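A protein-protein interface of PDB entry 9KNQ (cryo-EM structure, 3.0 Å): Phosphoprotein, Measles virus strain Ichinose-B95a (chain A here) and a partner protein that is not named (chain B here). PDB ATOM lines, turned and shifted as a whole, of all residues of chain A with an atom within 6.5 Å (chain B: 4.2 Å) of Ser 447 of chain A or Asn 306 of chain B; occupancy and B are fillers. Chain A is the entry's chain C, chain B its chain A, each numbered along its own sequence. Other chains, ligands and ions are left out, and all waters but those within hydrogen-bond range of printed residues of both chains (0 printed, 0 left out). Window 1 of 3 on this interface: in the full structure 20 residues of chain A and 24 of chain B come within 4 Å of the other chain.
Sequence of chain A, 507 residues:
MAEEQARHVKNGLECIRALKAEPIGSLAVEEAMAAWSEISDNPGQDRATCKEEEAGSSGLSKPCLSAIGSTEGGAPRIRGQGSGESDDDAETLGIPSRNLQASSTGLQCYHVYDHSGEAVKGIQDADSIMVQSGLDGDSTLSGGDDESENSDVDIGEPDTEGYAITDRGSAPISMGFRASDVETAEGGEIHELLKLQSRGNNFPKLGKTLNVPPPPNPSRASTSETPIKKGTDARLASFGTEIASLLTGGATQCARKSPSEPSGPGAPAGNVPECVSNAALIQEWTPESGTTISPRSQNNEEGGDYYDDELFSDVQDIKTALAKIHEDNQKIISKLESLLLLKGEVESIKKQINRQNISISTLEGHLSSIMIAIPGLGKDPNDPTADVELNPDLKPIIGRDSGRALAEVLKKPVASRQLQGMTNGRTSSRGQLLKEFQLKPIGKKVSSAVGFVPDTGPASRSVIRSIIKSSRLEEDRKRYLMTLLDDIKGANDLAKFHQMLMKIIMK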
ATOM      1  N   LYS A 440       8.092  25.765 -12.620  1.00  0.00           N
ATOM      2  CA  LYS A 440       7.617  25.928 -11.250  1.00  0.00           C
ATOM      3  C   LYS A 440       8.796  26.232 -10.336  1.00  0.00           C
ATOM      4  O   LYS A 440       9.753  25.451 -10.290  1.00  0.00           O
ATOM      5  CB  LYS A 440       6.890  24.669 -10.785  1.00  0.00           C
ATOM      6  CG  LYS A 440       6.114  24.770  -9.464  1.00  0.00           C
ATOM      7  CD  LYS A 440       6.998  24.733  -8.225  1.00  0.00           C
ATOM      8  CE  LYS A 440       6.210  24.325  -6.992  1.00  0.00           C
ATOM      9  NZ  LYS A 440       7.075  23.672  -5.972  1.00  0.00           N
ATOM     10  N   ILE A 442      11.205  26.461  -7.164  1.00  0.00           N
ATOM     11  CA  ILE A 442      11.461  25.666  -5.970  1.00  0.00           C
ATOM     12  C   ILE A 442      12.134  26.546  -4.927  1.00  0.00           C
ATOM     13  O   ILE A 442      13.139  27.209  -5.208  1.00  0.00           O
ATOM     14  CB  ILE A 442      12.309  24.425  -6.302  1.00  0.00           C
ATOM     15  CG1 ILE A 442      13.653  24.817  -6.912  1.00  0.00           C
ATOM     16  CG2 ILE A 442      11.555  23.508  -7.246  1.00  0.00           C
ATOM     17  CD1 ILE A 442      14.714  23.765  -6.759  1.00  0.00           C
ATOM     18  N   GLY A 443      11.558  26.580  -3.730  1.00  0.00           N
ATOM     19  CA  GLY A 443      12.101  27.383  -2.655  1.00  0.00           C
ATOM     20  C   GLY A 443      12.541  26.548  -1.474  1.00  0.00           C
ATOM     21  O   GLY A 443      12.981  25.406  -1.641  1.00  0.00           O
ATOM     22  N   LYS A 445      10.419  25.687   1.027  1.00  0.00           N
ATOM     23  CA  LYS A 445       9.173  25.277   1.653  1.00  0.00           C
ATOM     24  C   LYS A 445       8.663  23.926   1.180  1.00  0.00           C
ATOM     25  O   LYS A 445       7.961  23.254   1.942  1.00  0.00           O
ATOM     26  CB  LYS A 445       8.072  26.323   1.410  1.00  0.00           C
ATOM     27  CG  LYS A 445       8.302  27.665   2.091  1.00  0.00           C
ATOM     28  CD  LYS A 445       9.205  28.577   1.272  1.00  0.00           C
ATOM     29  CE  LYS A 445       8.913  28.459  -0.215  1.00  0.00           C
ATOM     30  NZ  LYS A 445       9.841  29.289  -1.025  1.00  0.00           N
ATOM     31  N   VAL A 446       8.983  23.511  -0.042  1.00  0.00           N
ATOM     32  CA  VAL A 446       8.625  22.192  -0.546  1.00  0.00           C
ATOM     33  C   VAL A 446       9.908  21.446  -0.883  1.00  0.00           C
ATOM     34  O   VAL A 446      10.893  22.049  -1.327  1.00  0.00           O
ATOM     35  CB  VAL A 446       7.683  22.272  -1.767  1.00  0.00           C
ATOM     36  CG1 VAL A 446       6.456  23.107  -1.435  1.00  0.00           C
ATOM     37  CG2 VAL A 446       8.402  22.849  -2.974  1.00  0.00           C
ATOM     38  N   SER A 447       9.901  20.138  -0.652  1.00  0.00           N
ATOM     39  CA  SER A 447      11.109  19.341  -0.794  1.00  0.00           C
ATOM     40  C   SER A 447      11.506  19.194  -2.257  1.00  0.00           C
ATOM     41  O   SER A 447      10.662  19.112  -3.152  1.00  0.00           O
ATOM     42  CB  SER A 447      10.916  17.961  -0.173  1.00  0.00           C
ATOM     43  OG  SER A 447      12.014  17.118  -0.470  1.00  0.00           O
ATOM     44  N   SER A 448      12.814  19.155  -2.489  1.00  0.00           N
ATOM     45  CA  SER A 448      13.363  18.950  -3.822  1.00  0.00           C
ATOM     46  C   SER A 448      14.777  18.403  -3.675  1.00  0.00           C
ATOM     47  O   SER A 448      15.262  18.176  -2.565  1.00  0.00           O
ATOM     48  CB  SER A 448      13.348  20.245  -4.633  1.00  0.00           C
ATOM     49  OG  SER A 448      14.129  20.110  -5.804  1.00  0.00           O
ATOM     50  N   ALA A 449      15.446  18.203  -4.812  1.00  0.00           N
ATOM     51  CA  ALA A 449      16.810  17.689  -4.791  1.00  0.00           C
ATOM     52  C   ALA A 449      17.783  18.625  -4.094  1.00  0.00           C
ATOM     53  O   ALA A 449      18.934  18.236  -3.868  1.00  0.00           O
ATOM     54  CB  ALA A 449      17.300  17.422  -6.212  1.00  0.00           C
ATOM     55  N   VAL A 450      17.359  19.839  -3.752  1.00  0.00           N
ATOM     56  CA  VAL A 450      18.240  20.780  -3.075  1.00  0.00           C
ATOM     57  C   VAL A 450      18.288  20.491  -1.582  1.00  0.00           C
ATOM     58  O   VAL A 450      19.364  20.432  -0.979  1.00  0.00           O
ATOM     59  CB  VAL A 450      17.781  22.221  -3.355  1.00  0.00           C
ATOM     60  CG1 VAL A 450      18.872  23.208  -3.017  1.00  0.00           C
ATOM     61  CG2 VAL A 450      17.380  22.364  -4.801  1.00  0.00           C
ATOM     62  N   GLY A 451      17.128  20.304  -0.967  1.00  0.00           N
ATOM     63  CA  GLY A 451      17.058  20.003   0.449  1.00  0.00           C
ATOM     64  C   GLY A 451      15.741  19.330   0.755  1.00  0.00           C
ATOM     65  O   GLY A 451      14.819  19.309  -0.063  1.00  0.00           O
ATOM     66  N   PHE A 452      15.658  18.777   1.958  1.00  0.00           N
ATOM     67  CA  PHE A 452      14.485  18.036   2.394  1.00  0.00           C
ATOM     68  C   PHE A 452      13.735  18.834   3.449  1.00  0.00           C
ATOM     69  O   PHE A 452      14.332  19.290   4.428  1.00  0.00           O
ATOM     70  CB  PHE A 452      14.879  16.668   2.948  1.00  0.00           C
ATOM     71  CG  PHE A 452      13.828  16.042   3.808  1.00  0.00           C
ATOM     72  CD1 PHE A 452      12.641  15.602   3.258  1.00  0.00           C
ATOM     73  CD2 PHE A 452      14.022  15.903   5.170  1.00  0.00           C
ATOM     74  CE1 PHE A 452      11.669  15.029   4.044  1.00  0.00           C
ATOM     75  CE2 PHE A 452      13.053  15.332   5.961  1.00  0.00           C
ATOM     76  CZ  PHE A 452      11.874  14.898   5.398  1.00  0.00           C
ATOM     77  N   VAL A 453      12.434  19.011   3.236  1.00  0.00           N
ATOM     78  CA  VAL A 453      11.548  19.594   4.239  1.00  0.00           C
ATOM     79  C   VAL A 453      10.323  18.696   4.376  1.00  0.00           C
ATOM     80  O   VAL A 453       9.760  18.254   3.363  1.00  0.00           O
ATOM     81  CB  VAL A 453      11.164  21.043   3.891  1.00  0.00           C
ATOM     82  CG1 VAL A 453      12.408  21.899   3.739  1.00  0.00           C
ATOM     83  CG2 VAL A 453      10.338  21.099   2.617  1.00  0.00           C
ATOM     84  N   PRO A 454       9.899  18.368   5.592  1.00  0.00           N
ATOM     85  CA  PRO A 454       8.756  17.466   5.762  1.00  0.00           C
ATOM     86  C   PRO A 454       7.456  18.126   5.330  1.00  0.00           C
ATOM     87  O   PRO A 454       7.382  19.328   5.073  1.00  0.00           O
ATOM     88  CB  PRO A 454       8.757  17.166   7.264  1.00  0.00           C
ATOM     89  CG  PRO A 454      10.124  17.551   7.737  1.00  0.00           C
ATOM     90  CD  PRO A 454      10.537  18.692   6.876  1.00  0.00           C
ATOM     91  N   ASP A 455       6.414  17.306   5.251  1.00  0.00           N
ATOM     92  CA  ASP A 455       5.081  17.774   4.897  1.00  0.00           C
ATOM     93  C   ASP A 455       4.067  16.766   5.427  1.00  0.00           C
ATOM     94  O   ASP A 455       4.400  15.887   6.228  1.00  0.00           O
ATOM     95  CB  ASP A 455       4.956  17.986   3.386  1.00  0.00           C
ATOM     96  CG  ASP A 455       4.985  16.690   2.617  1.00  0.00           C
ATOM     97  OD1 ASP A 455       5.841  15.836   2.927  1.00  0.00           O
ATOM     98  OD2 ASP A 455       4.146  16.521   1.707  1.00  0.00           O
ATOM     99  N   ALA A 459       5.051   9.906   3.150  1.00  0.00           N
ATOM    100  CA  ALA A 459       6.454   9.600   2.910  1.00  0.00           C
ATOM    101  C   ALA A 459       7.375  10.333   3.874  1.00  0.00           C
ATOM    102  O   ALA A 459       8.484   9.856   4.153  1.00  0.00           O
ATOM    103  CB  ALA A 459       6.828   9.943   1.470  1.00  0.00           C
ATOM    104  N   SER A 460       6.940  11.482   4.394  1.00  0.00           N
ATOM    105  CA  SER A 460       7.797  12.260   5.279  1.00  0.00           C
ATOM    106  C   SER A 460       8.027  11.543   6.602  1.00  0.00           C
ATOM    107  O   SER A 460       9.147  11.538   7.125  1.00  0.00           O
ATOM    108  CB  SER A 460       7.189  13.639   5.514  1.00  0.00           C
ATOM    109  OG  SER A 460       6.681  14.173   4.306  1.00  0.00           O
ATOM    110  N   VAL A 463      10.604   8.823   5.921  1.00  0.00           N
ATOM    111  CA  VAL A 463      11.985   9.266   5.749  1.00  0.00           C
ATOM    112  C   VAL A 463      12.553   9.787   7.064  1.00  0.00           C
ATOM    113  O   VAL A 463      13.753   9.637   7.328  1.00  0.00           O
ATOM    114  CB  VAL A 463      12.107  10.307   4.623  1.00  0.00           C
ATOM    115  CG1 VAL A 463      11.655   9.713   3.310  1.00  0.00           C
ATOM    116  CG2 VAL A 463      11.306  11.529   4.938  1.00  0.00           C
ATOM    117  N   GLY B 302      18.128  12.665   2.944  1.00  0.00           N
ATOM    118  CA  GLY B 302      16.754  12.312   2.651  1.00  0.00           C
ATOM    119  C   GLY B 302      16.188  12.903   1.380  1.00  0.00           C
ATOM    120  O   GLY B 302      15.036  12.602   1.042  1.00  0.00           O
ATOM    121  N   ALA B 303      16.957  13.717   0.655  1.00  0.00           N
ATOM    122  CA  ALA B 303      16.425  14.404  -0.517  1.00  0.00           C
ATOM    123  C   ALA B 303      15.916  13.418  -1.561  1.00  0.00           C
ATOM    124  O   ALA B 303      14.769  13.508  -2.009  1.00  0.00           O
ATOM    125  CB  ALA B 303      17.495  15.314  -1.113  1.00  0.00           C
ATOM    126  N   PHE B 304      16.760  12.471  -1.964  1.00  0.00           N
ATOM    127  CA  PHE B 304      16.368  11.500  -2.978  1.00  0.00           C
ATOM    128  C   PHE B 304      15.420  10.446  -2.419  1.00  0.00           C
ATOM    129  O   PHE B 304      14.527   9.969  -3.136  1.00  0.00           O
ATOM    130  CB  PHE B 304      17.621  10.842  -3.556  1.00  0.00           C
ATOM    131  CG  PHE B 304      17.444  10.296  -4.937  1.00  0.00           C
ATOM    132  CD1 PHE B 304      16.350  10.641  -5.702  1.00  0.00           C
ATOM    133  CD2 PHE B 304      18.382   9.436  -5.472  1.00  0.00           C
ATOM    134  CE1 PHE B 304      16.195  10.135  -6.971  1.00  0.00           C
ATOM    135  CE2 PHE B 304      18.231   8.928  -6.738  1.00  0.00           C
ATOM    136  CZ  PHE B 304      17.137   9.277  -7.489  1.00  0.00           C
ATOM    137  N   LEU B 305      15.604  10.073  -1.152  1.00  0.00           N
ATOM    138  CA  LEU B 305      14.742   9.078  -0.530  1.00  0.00           C
ATOM    139  C   LEU B 305      13.295   9.549  -0.489  1.00  0.00           C
ATOM    140  O   LEU B 305      12.366   8.753  -0.677  1.00  0.00           O
ATOM    141  CB  LEU B 305      15.250   8.769   0.876  1.00  0.00           C
ATOM    142  CG  LEU B 305      14.635   7.576   1.597  1.00  0.00           C
ATOM    143  CD1 LEU B 305      14.848   6.312   0.793  1.00  0.00           C
ATOM    144  CD2 LEU B 305      15.235   7.438   2.979  1.00  0.00           C
ATOM    145  N   ASN B 306      13.083  10.843  -0.238  1.00  0.00           N
ATOM    146  CA  ASN B 306      11.731  11.381  -0.200  1.00  0.00           C
ATOM    147  C   ASN B 306      11.017  11.224  -1.532  1.00  0.00           C
ATOM    148  O   ASN B 306       9.784  11.183  -1.563  1.00  0.00           O
ATOM    149  CB  ASN B 306      11.769  12.851   0.211  1.00  0.00           C
ATOM    150  CG  ASN B 306      10.429  13.533   0.060  1.00  0.00           C
ATOM    151  OD1 ASN B 306       9.595  13.491   0.959  1.00  0.00           O
ATOM    152  ND2 ASN B 306      10.216  14.169  -1.083  1.00  0.00           N
ATOM    153  N   HIS B 307      11.760  11.124  -2.630  1.00  0.00           N
ATOM    154  CA  HIS B 307      11.149  10.902  -3.932  1.00  0.00           C
ATOM    155  C   HIS B 307      10.971   9.424  -4.235  1.00  0.00           C
ATOM    156  O   HIS B 307       9.939   9.024  -4.792  1.00  0.00           O
ATOM    157  CB  HIS B 307      11.992  11.544  -5.032  1.00  0.00           C
ATOM    158  CG  HIS B 307      11.632  11.084  -6.408  1.00  0.00           C
ATOM    159  ND1 HIS B 307      10.383  11.283  -6.955  1.00  0.00           N
ATOM    160  CD2 HIS B 307      12.351  10.422  -7.344  1.00  0.00           C
ATOM    161  CE1 HIS B 307      10.350  10.771  -8.172  1.00  0.00           C
ATOM    162  NE2 HIS B 307      11.532  10.243  -8.433  1.00  0.00           N
ATOM    163  N   CYS B 308      11.971   8.605  -3.899  1.00  0.00           N
ATOM    164  CA  CYS B 308      11.835   7.170  -4.132  1.00  0.00           C
ATOM    165  C   CYS B 308      10.643   6.599  -3.371  1.00  0.00           C
ATOM    166  O   CYS B 308       9.881   5.788  -3.914  1.00  0.00           O
ATOM    167  CB  CYS B 308      13.118   6.431  -3.757  1.00  0.00           C
ATOM    168  SG  CYS B 308      14.642   7.183  -4.349  1.00  0.00           S
ATOM    169  N   THR B 310       7.918   8.186  -2.411  1.00  0.00           N
ATOM    170  CA  THR B 310       6.685   8.644  -3.042  1.00  0.00           C
ATOM    171  C   THR B 310       6.375   7.829  -4.288  1.00  0.00           C
ATOM    172  O   THR B 310       5.224   7.435  -4.514  1.00  0.00           O
ATOM    173  CB  THR B 310       6.789  10.125  -3.392  1.00  0.00           C
ATOM    174  OG1 THR B 310       7.005  10.884  -2.199  1.00  0.00           O
ATOM    175  CG2 THR B 310       5.513  10.600  -4.059  1.00  0.00           C
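Of chain A, only Ser 447 and Val 463 come within 4 Å of Asn 306 of chain B. Printed residues of chain B within 4 Å of Ala 459 of chain A: Thr 310. Of the printed residues of chain A, Ala 303 of chain B touches Ser 448 (3.9 Å). Ile 442 of chain A touches none of the printed residues of chain B. The nearest printed residue of chain B that does not touch Ser 447 of chain A is Ala 303 of chain B (4.8 Å).
The backbone carbonyl oxygen of Asn 306 of chain B lies within hydrogen-bond range of the side-chain hydroxyl of Thr 310 of chain B (2.9 Å).
Among the printed residues, merely in contact across the chains: Ser 447 of chain A with Asn 306 of chain B (3.5 Å), Ala 459 of chain A with Thr 310 of chain B (3.8 Å), Val 463 of chain A with Asn 306 of chain B (3.9 Å) and Ser 448 of chain A with Ala 303 of chain B (3.9 Å).
Of the 8 printed residues of chain B, 3 touch a printed residue of chain A. Hydrophobic or aromatic side chains of chain B that line the printed part of chain A: Ala 303. Of the 17 printed residues of chain A, 4 touch a printed residue of chain B. Hydrophobic or aromatic side chains of chain A that line the printed part of chain B: Ala 459 and Val 463. Among the printed residues, 4 pairs touch across the chains.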
